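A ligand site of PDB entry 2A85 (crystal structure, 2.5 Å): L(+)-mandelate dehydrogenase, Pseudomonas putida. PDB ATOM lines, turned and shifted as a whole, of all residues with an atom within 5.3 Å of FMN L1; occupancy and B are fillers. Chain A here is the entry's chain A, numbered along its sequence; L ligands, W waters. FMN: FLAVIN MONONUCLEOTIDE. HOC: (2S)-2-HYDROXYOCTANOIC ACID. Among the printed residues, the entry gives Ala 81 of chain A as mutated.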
ATOM      1  N   TYR A  26      20.906  10.267   3.327  1.00  0.00           N
ATOM      2  CA  TYR A  26      19.564  10.323   3.906  1.00  0.00           C
ATOM      3  C   TYR A  26      18.928   8.936   3.812  1.00  0.00           C
ATOM      4  O   TYR A  26      18.301   8.448   4.757  1.00  0.00           O
ATOM      5  CB  TYR A  26      18.685  11.314   3.138  1.00  0.00           C
ATOM      6  CG  TYR A  26      17.199  11.098   3.363  1.00  0.00           C
ATOM      7  CD1 TYR A  26      16.607  11.428   4.585  1.00  0.00           C
ATOM      8  CD2 TYR A  26      16.398  10.545   2.363  1.00  0.00           C
ATOM      9  CE1 TYR A  26      15.254  11.198   4.806  1.00  0.00           C
ATOM     10  CE2 TYR A  26      15.040  10.312   2.576  1.00  0.00           C
ATOM     11  CZ  TYR A  26      14.476  10.640   3.791  1.00  0.00           C
ATOM     12  OH  TYR A  26      13.129  10.416   4.006  1.00  0.00           O
ATOM     13  N   LEU A  27      19.111   8.293   2.660  1.00  0.00           N
ATOM     14  CA  LEU A  27      18.572   6.981   2.379  1.00  0.00           C
ATOM     15  C   LEU A  27      19.234   5.839   3.151  1.00  0.00           C
ATOM     16  O   LEU A  27      18.556   5.064   3.832  1.00  0.00           O
ATOM     17  CB  LEU A  27      18.708   6.712   0.867  1.00  0.00           C
ATOM     18  CG  LEU A  27      18.558   5.296   0.309  1.00  0.00           C
ATOM     19  CD1 LEU A  27      17.159   4.774   0.547  1.00  0.00           C
ATOM     20  CD2 LEU A  27      18.878   5.328  -1.182  1.00  0.00           C
ATOM     21  N   GLY A  78       7.240  -1.115   1.320  1.00  0.00           N
ATOM     22  CA  GLY A  78       6.853  -0.381   2.513  1.00  0.00           C
ATOM     23  C   GLY A  78       6.840   1.121   2.403  1.00  0.00           C
ATOM     24  O   GLY A  78       7.379   1.696   1.455  1.00  0.00           O
ATOM     25  N   PRO A  79       6.224   1.807   3.369  1.00  0.00           N
ATOM     26  CA  PRO A  79       6.148   3.262   3.372  1.00  0.00           C
ATOM     27  C   PRO A  79       7.485   3.938   3.680  1.00  0.00           C
ATOM     28  O   PRO A  79       8.124   3.663   4.705  1.00  0.00           O
ATOM     29  CB  PRO A  79       5.084   3.552   4.427  1.00  0.00           C
ATOM     30  CG  PRO A  79       5.352   2.455   5.435  1.00  0.00           C
ATOM     31  CD  PRO A  79       5.534   1.245   4.552  1.00  0.00           C
ATOM     32  N   THR A  80       7.903   4.805   2.774  1.00  0.00           N
ATOM     33  CA  THR A  80       9.129   5.554   2.947  1.00  0.00           C
ATOM     34  C   THR A  80       8.882   6.968   2.485  1.00  0.00           C
ATOM     35  O   THR A  80       8.204   7.212   1.462  1.00  0.00           O
ATOM     36  CB  THR A  80      10.303   4.955   2.171  1.00  0.00           C
ATOM     37  OG1 THR A  80       9.924   4.737   0.802  1.00  0.00           O
ATOM     38  CG2 THR A  80      10.738   3.645   2.807  1.00  0.00           C
ATOM     39  N   ALA A  81       9.416   7.897   3.284  1.00  0.00           N
ATOM     40  CA  ALA A  81       9.272   9.337   3.060  1.00  0.00           C
ATOM     41  C   ALA A  81      10.250   9.901   2.050  1.00  0.00           C
ATOM     42  O   ALA A  81      11.342   9.352   1.872  1.00  0.00           O
ATOM     43  CB  ALA A  81       9.444  10.109   4.383  1.00  0.00           C
ATOM     44  N   SER A 108       3.493   6.789   2.141  1.00  0.00           N
ATOM     45  CA  SER A 108       3.917   7.412   3.381  1.00  0.00           C
ATOM     46  C   SER A 108       3.134   8.698   3.638  1.00  0.00           C
ATOM     47  O   SER A 108       2.700   9.376   2.700  1.00  0.00           O
ATOM     48  CB  SER A 108       5.412   7.717   3.313  1.00  0.00           C
ATOM     49  OG  SER A 108       5.809   8.546   4.387  1.00  0.00           O
ATOM     50  N   THR A 109       2.945   9.030   4.910  1.00  0.00           N
ATOM     51  CA  THR A 109       2.256  10.259   5.285  1.00  0.00           C
ATOM     52  C   THR A 109       3.066  11.403   4.705  1.00  0.00           C
ATOM     53  O   THR A 109       2.515  12.418   4.266  1.00  0.00           O
ATOM     54  CB  THR A 109       2.192  10.425   6.818  1.00  0.00           C
ATOM     55  OG1 THR A 109       1.233   9.509   7.354  1.00  0.00           O
ATOM     56  CG2 THR A 109       1.804  11.845   7.190  1.00  0.00           C
ATOM     57  N   ALA A 110       4.386  11.229   4.708  1.00  0.00           N
ATOM     58  CA  ALA A 110       5.308  12.241   4.193  1.00  0.00           C
ATOM     59  C   ALA A 110       5.772  11.961   2.764  1.00  0.00           C
ATOM     60  O   ALA A 110       6.967  12.026   2.458  1.00  0.00           O
ATOM     61  CB  ALA A 110       6.516  12.341   5.123  1.00  0.00           C
ATOM     62  N   GLN A 129       0.150   4.732   5.091  1.00  0.00           N
ATOM     63  CA  GLN A 129       0.829   4.739   6.364  1.00  0.00           C
ATOM     64  C   GLN A 129       0.546   6.083   6.979  1.00  0.00           C
ATOM     65  O   GLN A 129       0.775   7.104   6.352  1.00  0.00           O
ATOM     66  CB  GLN A 129       2.334   4.557   6.169  1.00  0.00           C
ATOM     67  CG  GLN A 129       3.177   4.755   7.425  1.00  0.00           C
ATOM     68  CD  GLN A 129       3.638   6.190   7.632  1.00  0.00           C
ATOM     69  OE1 GLN A 129       3.399   6.788   8.672  1.00  0.00           O
ATOM     70  NE2 GLN A 129       4.293   6.749   6.629  1.00  0.00           N
ATOM     71  N   TYR A 131       1.065   8.979  10.032  1.00  0.00           N
ATOM     72  CA  TYR A 131       1.883   9.571  11.083  1.00  0.00           C
ATOM     73  C   TYR A 131       0.925  10.613  11.679  1.00  0.00           C
ATOM     74  O   TYR A 131       0.237  11.301  10.924  1.00  0.00           O
ATOM     75  CB  TYR A 131       3.099  10.306  10.523  1.00  0.00           C
ATOM     76  CG  TYR A 131       4.346   9.482  10.335  1.00  0.00           C
ATOM     77  CD1 TYR A 131       4.744   8.554  11.306  1.00  0.00           C
ATOM     78  CD2 TYR A 131       5.170   9.680   9.240  1.00  0.00           C
ATOM     79  CE1 TYR A 131       5.936   7.854  11.182  1.00  0.00           C
ATOM     80  CE2 TYR A 131       6.368   8.988   9.096  1.00  0.00           C
ATOM     81  CZ  TYR A 131       6.742   8.079  10.078  1.00  0.00           C
ATOM     82  OH  TYR A 131       7.945   7.424   9.956  1.00  0.00           O
ATOM     83  N   THR A 156       2.090   4.039  12.098  1.00  0.00           N
ATOM     84  CA  THR A 156       3.513   3.881  12.444  1.00  0.00           C
ATOM     85  C   THR A 156       3.711   4.524  13.804  1.00  0.00           C
ATOM     86  O   THR A 156       3.433   5.699  13.986  1.00  0.00           O
ATOM     87  CB  THR A 156       4.420   4.558  11.423  1.00  0.00           C
ATOM     88  OG1 THR A 156       4.157   3.990  10.137  1.00  0.00           O
ATOM     89  CG2 THR A 156       5.890   4.334  11.769  1.00  0.00           C
ATOM     90  N   LYS A 231       2.429  -0.563  12.922  1.00  0.00           N
ATOM     91  CA  LYS A 231       3.825  -0.738  12.548  1.00  0.00           C
ATOM     92  C   LYS A 231       4.787  -0.118  13.562  1.00  0.00           C
ATOM     93  O   LYS A 231       4.505   0.918  14.140  1.00  0.00           O
ATOM     94  CB  LYS A 231       4.034  -0.091  11.175  1.00  0.00           C
ATOM     95  CG  LYS A 231       5.467  -0.064  10.642  1.00  0.00           C
ATOM     96  CD  LYS A 231       5.445   0.319   9.155  1.00  0.00           C
ATOM     97  CE  LYS A 231       6.837   0.377   8.514  1.00  0.00           C
ATOM     98  NZ  LYS A 231       7.603   1.598   8.890  1.00  0.00           N
ATOM     99  N   SER A 253       8.984  -4.109  13.510  1.00  0.00           N
ATOM    100  CA  SER A 253       9.939  -3.286  12.803  1.00  0.00           C
ATOM    101  C   SER A 253      10.704  -2.349  13.726  1.00  0.00           C
ATOM    102  O   SER A 253      10.180  -1.955  14.774  1.00  0.00           O
ATOM    103  CB  SER A 253       9.163  -2.463  11.759  1.00  0.00           C
ATOM    104  OG  SER A 253       9.886  -1.329  11.336  1.00  0.00           O
ATOM    105  N   HIS A 255      12.242   0.301  12.195  1.00  0.00           N
ATOM    106  CA  HIS A 255      12.384   1.392  11.236  1.00  0.00           C
ATOM    107  C   HIS A 255      13.663   1.326  10.424  1.00  0.00           C
ATOM    108  O   HIS A 255      14.214   2.366  10.068  1.00  0.00           O
ATOM    109  CB  HIS A 255      12.338   2.722  11.979  1.00  0.00           C
ATOM    110  CG  HIS A 255      11.521   3.772  11.274  1.00  0.00           C
ATOM    111  ND1 HIS A 255      10.162   3.890  11.447  1.00  0.00           N
ATOM    112  CD2 HIS A 255      11.879   4.739  10.403  1.00  0.00           C
ATOM    113  CE1 HIS A 255       9.716   4.895  10.717  1.00  0.00           C
ATOM    114  NE2 HIS A 255      10.740   5.427  10.069  1.00  0.00           N
ATOM    115  N   GLY A 256      14.121   0.122  10.120  1.00  0.00           N
ATOM    116  CA  GLY A 256      15.332  -0.012   9.329  1.00  0.00           C
ATOM    117  C   GLY A 256      16.537   0.579  10.032  1.00  0.00           C
ATOM    118  O   GLY A 256      17.410   1.152   9.379  1.00  0.00           O
ATOM    119  N   ARG A 258      16.844   3.207  11.827  1.00  0.00           N
ATOM    120  CA  ARG A 258      16.925   4.653  11.769  1.00  0.00           C
ATOM    121  C   ARG A 258      16.405   5.408  12.989  1.00  0.00           C
ATOM    122  O   ARG A 258      16.606   6.615  13.104  1.00  0.00           O
ATOM    123  CB  ARG A 258      16.173   5.144  10.524  1.00  0.00           C
ATOM    124  CG  ARG A 258      16.741   4.596   9.226  1.00  0.00           C
ATOM    125  CD  ARG A 258      15.726   4.646   8.103  1.00  0.00           C
ATOM    126  NE  ARG A 258      15.411   5.997   7.635  1.00  0.00           N
ATOM    127  CZ  ARG A 258      16.195   6.712   6.833  1.00  0.00           C
ATOM    128  NH1 ARG A 258      17.349   6.213   6.412  1.00  0.00           N
ATOM    129  NH2 ARG A 258      15.814   7.911   6.426  1.00  0.00           N
ATOM    130  N   ASP A 284       9.658  -6.089   8.684  1.00  0.00           N
ATOM    131  CA  ASP A 284      10.628  -5.411   7.823  1.00  0.00           C
ATOM    132  C   ASP A 284      11.843  -5.081   8.658  1.00  0.00           C
ATOM    133  O   ASP A 284      11.870  -5.385   9.858  1.00  0.00           O
ATOM    134  CB  ASP A 284      10.049  -4.133   7.188  1.00  0.00           C
ATOM    135  CG  ASP A 284       9.862  -2.977   8.182  1.00  0.00           C
ATOM    136  OD1 ASP A 284      10.626  -2.865   9.152  1.00  0.00           O
ATOM    137  OD2 ASP A 284       8.939  -2.162   7.955  1.00  0.00           O
ATOM    138  N   SER A 285      12.837  -4.472   8.020  1.00  0.00           N
ATOM    139  CA  SER A 285      14.092  -4.047   8.665  1.00  0.00           C
ATOM    140  C   SER A 285      15.272  -4.981   8.462  1.00  0.00           C
ATOM    141  O   SER A 285      15.469  -5.927   9.227  1.00  0.00           O
ATOM    142  CB  SER A 285      13.893  -3.798  10.166  1.00  0.00           C
ATOM    143  OG  SER A 285      13.028  -2.687  10.415  1.00  0.00           O
ATOM    144  N   GLY A 286      16.048  -4.715   7.418  1.00  0.00           N
ATOM    145  CA  GLY A 286      17.220  -5.515   7.149  1.00  0.00           C
ATOM    146  C   GLY A 286      17.149  -6.455   5.963  1.00  0.00           C
ATOM    147  O   GLY A 286      18.182  -6.971   5.545  1.00  0.00           O
ATOM    148  N   PHE A 287      15.959  -6.662   5.414  1.00  0.00           N
ATOM    149  CA  PHE A 287      15.789  -7.577   4.292  1.00  0.00           C
ATOM    150  C   PHE A 287      16.418  -7.121   2.971  1.00  0.00           C
ATOM    151  O   PHE A 287      16.091  -6.057   2.441  1.00  0.00           O
ATOM    152  CB  PHE A 287      14.300  -7.870   4.095  1.00  0.00           C
ATOM    153  CG  PHE A 287      13.664  -8.553   5.266  1.00  0.00           C
ATOM    154  CD1 PHE A 287      13.272  -7.821   6.386  1.00  0.00           C
ATOM    155  CD2 PHE A 287      13.473  -9.931   5.266  1.00  0.00           C
ATOM    156  CE1 PHE A 287      12.676  -8.448   7.497  1.00  0.00           C
ATOM    157  CE2 PHE A 287      12.877 -10.569   6.367  1.00  0.00           C
ATOM    158  CZ  PHE A 287      12.484  -9.837   7.487  1.00  0.00           C
ATOM    159  N   ARG A 288      17.325  -7.949   2.443  1.00  0.00           N
ATOM    160  CA  ARG A 288      18.008  -7.646   1.198  1.00  0.00           C
ATOM    161  C   ARG A 288      18.081  -8.868   0.284  1.00  0.00           C
ATOM    162  O   ARG A 288      18.070  -8.750  -0.942  1.00  0.00           O
ATOM    163  CB  ARG A 288      19.424  -7.164   1.501  1.00  0.00           C
ATOM    164  CG  ARG A 288      19.508  -5.969   2.438  1.00  0.00           C
ATOM    165  CD  ARG A 288      19.183  -4.674   1.727  1.00  0.00           C
ATOM    166  NE  ARG A 288      19.378  -3.537   2.615  1.00  0.00           N
ATOM    167  CZ  ARG A 288      18.591  -3.250   3.648  1.00  0.00           C
ATOM    168  NH1 ARG A 288      17.525  -4.009   3.913  1.00  0.00           N
ATOM    169  NH2 ARG A 288      18.886  -2.215   4.420  1.00  0.00           N
ATOM    170  N   LEU A 305       7.948  -6.456   4.255  1.00  0.00           N
ATOM    171  CA  LEU A 305       7.877  -5.157   3.587  1.00  0.00           C
ATOM    172  C   LEU A 305       9.295  -4.733   3.227  1.00  0.00           C
ATOM    173  O   LEU A 305      10.227  -4.910   4.004  1.00  0.00           O
ATOM    174  CB  LEU A 305       7.230  -4.099   4.489  1.00  0.00           C
ATOM    175  CG  LEU A 305       5.760  -4.269   4.904  1.00  0.00           C
ATOM    176  CD1 LEU A 305       5.678  -5.200   6.100  1.00  0.00           C
ATOM    177  CD2 LEU A 305       5.160  -2.920   5.276  1.00  0.00           C
ATOM    178  N   LEU A 306       9.454  -4.200   2.032  1.00  0.00           N
ATOM    179  CA  LEU A 306      10.757  -3.758   1.596  1.00  0.00           C
ATOM    180  C   LEU A 306      10.917  -2.264   1.773  1.00  0.00           C
ATOM    181  O   LEU A 306      10.013  -1.468   1.462  1.00  0.00           O
ATOM    182  CB  LEU A 306      10.975  -4.125   0.121  1.00  0.00           C
ATOM    183  CG  LEU A 306      11.052  -5.623  -0.151  1.00  0.00           C
ATOM    184  CD1 LEU A 306      11.193  -5.865  -1.651  1.00  0.00           C
ATOM    185  CD2 LEU A 306      12.241  -6.215   0.615  1.00  0.00           C
ATOM    186  N   GLY A 307      12.069  -1.881   2.316  1.00  0.00           N
ATOM    187  CA  GLY A 307      12.376  -0.484   2.507  1.00  0.00           C
ATOM    188  C   GLY A 307      13.437  -0.063   1.510  1.00  0.00           C
ATOM    189  O   GLY A 307      13.139   0.242   0.354  1.00  0.00           O
ATOM    190  N   ARG A 308      14.690  -0.090   1.950  1.00  0.00           N
ATOM    191  CA  ARG A 308      15.804   0.309   1.115  1.00  0.00           C
ATOM    192  C   ARG A 308      16.026  -0.533  -0.152  1.00  0.00           C
ATOM    193  O   ARG A 308      16.398   0.010  -1.186  1.00  0.00           O
ATOM    194  CB  ARG A 308      17.107   0.338   1.936  1.00  0.00           C
ATOM    195  CG  ARG A 308      17.113   1.356   3.066  1.00  0.00           C
ATOM    196  CD  ARG A 308      18.539   1.621   3.525  1.00  0.00           C
ATOM    197  NE  ARG A 308      18.620   2.362   4.784  1.00  0.00           N
ATOM    198  CZ  ARG A 308      18.222   1.906   5.974  1.00  0.00           C
ATOM    199  NH1 ARG A 308      17.692   0.692   6.090  1.00  0.00           N
ATOM    200  NH2 ARG A 308      18.407   2.637   7.057  1.00  0.00           N
ATOM    201  N   ALA A 309      15.798  -1.842  -0.072  1.00  0.00           N
ATOM    202  CA  ALA A 309      15.991  -2.716  -1.229  1.00  0.00           C
ATOM    203  C   ALA A 309      15.376  -2.142  -2.500  1.00  0.00           C
ATOM    204  O   ALA A 309      16.095  -1.897  -3.469  1.00  0.00           O
ATOM    205  CB  ALA A 309      15.406  -4.095  -0.954  1.00  0.00           C
ATOM    206  N   LEU A 311      14.156   0.820  -2.872  1.00  0.00           N
ATOM    207  CA  LEU A 311      14.562   2.210  -3.059  1.00  0.00           C
ATOM    208  C   LEU A 311      15.872   2.302  -3.845  1.00  0.00           C
ATOM    209  O   LEU A 311      16.119   3.308  -4.518  1.00  0.00           O
ATOM    210  CB  LEU A 311      14.706   2.932  -1.725  1.00  0.00           C
ATOM    211  CG  LEU A 311      13.393   3.256  -0.986  1.00  0.00           C
ATOM    212  CD1 LEU A 311      13.679   4.142   0.202  1.00  0.00           C
ATOM    213  CD2 LEU A 311      12.422   3.949  -1.934  1.00  0.00           C
HETATM  214  N1  FMN L   1       8.337   4.235   7.851  1.00  0.00           N
HETATM  215  C2  FMN L   1       7.062   4.763   7.953  1.00  0.00           C
HETATM  216  O2  FMN L   1       6.205   4.219   8.532  1.00  0.00           O
HETATM  217  N3  FMN L   1       6.807   6.030   7.264  1.00  0.00           N
HETATM  218  C4  FMN L   1       7.763   6.798   6.523  1.00  0.00           C
HETATM  219  O4  FMN L   1       7.500   7.853   5.963  1.00  0.00           O
HETATM  220  C4A FMN L   1       9.132   6.199   6.427  1.00  0.00           C
HETATM  221  N5  FMN L   1      10.126   6.796   5.729  1.00  0.00           N
HETATM  222  C5A FMN L   1      11.375   6.189   5.545  1.00  0.00           C
HETATM  223  C6  FMN L   1      12.380   6.816   4.687  1.00  0.00           C
HETATM  224  C7  FMN L   1      13.659   6.162   4.355  1.00  0.00           C
HETATM  225  C7M FMN L   1      14.610   6.886   3.452  1.00  0.00           C
HETATM  226  C8  FMN L   1      13.957   4.773   4.938  1.00  0.00           C
HETATM  227  C8M FMN L   1      15.215   3.978   4.655  1.00  0.00           C
HETATM  228  C9  FMN L   1      12.979   4.192   5.798  1.00  0.00           C
HETATM  229  C9A FMN L   1      11.673   4.810   6.137  1.00  0.00           C
HETATM  230  N10 FMN L   1      10.579   4.238   6.964  1.00  0.00           N
HETATM  231  C10 FMN L   1       9.302   4.860   7.151  1.00  0.00           C
HETATM  232  C1' FMN L   1      10.785   2.877   7.502  1.00  0.00           C
HETATM  233  C2' FMN L   1      10.398   1.820   6.458  1.00  0.00           C
HETATM  234  O2' FMN L   1       9.043   1.754   6.266  1.00  0.00           O
HETATM  235  C3' FMN L   1      10.899   0.411   6.783  1.00  0.00           C
HETATM  236  O3' FMN L   1      10.454   0.043   8.159  1.00  0.00           O
HETATM  237  C4' FMN L   1      12.410   0.225   6.804  1.00  0.00           C
HETATM  238  O4' FMN L   1      13.041   0.826   5.703  1.00  0.00           O
HETATM  239  C5' FMN L   1      12.717  -1.245   6.791  1.00  0.00           C
HETATM  240  O5' FMN L   1      14.155  -1.521   6.678  1.00  0.00           O
HETATM  241  P   FMN L   1      15.051  -1.745   5.441  1.00  0.00           P
HETATM  242  O1P FMN L   1      16.351  -2.391   5.849  1.00  0.00           O
HETATM  243  O2P FMN L   1      15.228  -0.418   4.801  1.00  0.00           O
HETATM  244  O3P FMN L   1      14.200  -2.661   4.588  1.00  0.00           O
HETATM  245  C8  HOC L   2      14.253  11.132  12.346  1.00  0.00           C
HETATM  246  C7  HOC L   2      13.174  12.014  11.735  1.00  0.00           C
HETATM  247  OH  HOC L   2      10.470   7.504   8.760  1.00  0.00           O
HETATM  248  C1  HOC L   2      12.338   8.847   8.017  1.00  0.00           C
HETATM  249  C2  HOC L   2      10.774   8.786   8.247  1.00  0.00           C
HETATM  250  C3  HOC L   2      10.163   9.797   9.254  1.00  0.00           C
HETATM  251  C4  HOC L   2      10.335  11.309   8.979  1.00  0.00           C
HETATM  252  C5  HOC L   2      11.189  12.095  10.029  1.00  0.00           C
HETATM  253  C6  HOC L   2      12.319  11.274  10.710  1.00  0.00           C
HETATM  254  O1A HOC L   2      13.044   7.862   8.679  1.00  0.00           O
HETATM  255  O1B HOC L   2      12.936   9.655   7.308  1.00  0.00           O
HETATM  256  O   HOH W   1      14.472  -3.331   2.121  1.00  0.00           O
HETATM  257  O   HOH W   2      12.750  -4.740   5.141  1.00  0.00           O
HETATM  258  O   HOH W   3       7.847  -0.738   5.566  1.00  0.00           O
HETATM  259  O   HOH W   4      17.822  -1.980   8.422  1.00  0.00           O
HETATM  260  O   HOH W   5      13.064   7.683   0.554  1.00  0.00           O
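The side-chain amino group (NZ) of Lys 231 sits at hydrogen-bond distance from a nitrogen (N1) of FMN L1, at 2.9 Å. The side-chain amide nitrogen of Gln 129 lies close to a nitrogen (N3) of FMN L1 (2.7 Å). O3P of FMN L1 lies within hydrogen-bond range of N of Gly 307, at 3.2 Å. O4 of FMN L1 is in hydrogen-bond range of OG of Ser 108, at 2.4 Å. A nitrogen (N3) of FMN L1 is in hydrogen-bond range of the side-chain hydroxyl (OH) of Tyr 131. The backbone NH of Arg 308 is in hydrogen-bond range of an oxygen (O2P) of FMN L1 (2.9 Å). NH1 of Arg 308 is in salt-bridge range of O2P of FMN L1 (3.0 Å). A nitrogen (N1) of FMN L1 lies close to a ring nitrogen (NE2) of His 255 (3.5 Å). The side-chain hydroxyl (OH) of Tyr 26 lies within hydrogen-bond range of an oxygen (O1B) of HOC L2 (3.4 Å). OD2 of Asp 284 sits at hydrogen-bond distance from O3' of FMN L1. The backbone carbonyl oxygen of Pro 79 is in hydrogen-bond range of an oxygen (O2') of FMN L1 (2.6 Å). An oxygen (O1P) of FMN L1 is in salt-bridge range of the guanidinium group (NH1) of Arg 288, 2.8 Å away. The side-chain hydroxyl of Thr 156 is in hydrogen-bond range of an oxygen (O2) of FMN L1 (2.6 Å). OH of HOC L2 sits at hydrogen-bond distance from OH of Tyr 131 (2.8 Å). O1P of FMN L1 sits at hydrogen-bond distance from N of Gly 286. NE2 of His 255 sits at hydrogen-bond distance from OH of HOC L2. N of Ala 81 is in hydrogen-bond range of N5 of FMN L1. O1A of HOC L2 lies within salt-bridge range of NE of Arg 258 (3.2 Å).
A nitrogen (N5) of FMN L1 sits close to an oxygen (OH) of HOC L2 (3.1 Å).
The backbone carbonyl oxygen (O) of Leu 27 is in hydrogen-bond range of the guanidinium group (NE) of Arg 308. The side-chain hydroxyl (OG) of Ser 108 is in hydrogen-bond range of the side-chain amide nitrogen (NE2) of Gln 129. The backbone carbonyl oxygen (O) of Gln 129 lies within hydrogen-bond range of the side-chain hydroxyl (OG1) of Thr 109, 2.6 Å away. The guanidinium group of Arg 288 lies close to the backbone carbonyl oxygen of Gly 286, 3.4 Å away. OG of Ser 108 lies close to N of Ala 110. The backbone NH (N) of Tyr 131 sits at hydrogen-bond distance from the side-chain hydroxyl (OG1) of Thr 109 (2.7 Å). A ring nitrogen (NE2) of His 255 lies close to the side-chain hydroxyl (OH) of Tyr 131 (3.4 Å). The backbone carbonyl oxygen (O) of Ala 81 sits at hydrogen-bond distance from the side-chain hydroxyl (OH) of Tyr 26 (3.0 Å).
N of Ser 285 lies close to O5' of FMN L1 (3.5 Å). Tyr 26 touches FMN L1 (CE2 to C7M, 3.6 Å). Leu 27 touches FMN L1. CA of Thr 80 touches N5 of FMN L1, at 3.2 Å. Ser 253 touches FMN L1. Gly 256 touches FMN L1 (CA to O5', 3.3 Å). Arg 258 touches FMN L1 (NE to C8, 3.3 Å). Hydrophobic or aromatic side chains within 4 Å of FMN L1: Tyr 26, Pro 79, Ala 81, Tyr 131 and His 255. The nearest printed residue that does not touch FMN L1 is Phe 287 (4.3 Å).
Water W2 lies within hydrogen-bond range of O3P of FMN L1 (2.6 Å), O of Leu 305 (2.8 Å) and N of Ser 285 (2.9 Å). Water W3 bridges an oxygen (O2') of FMN L1 (2.9 Å) and the side-chain carboxylate of Asp 284 (3.0 Å). Water W4 lies within hydrogen-bond range of O1P of FMN L1, O of Gly 256 and N of Gly 286.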
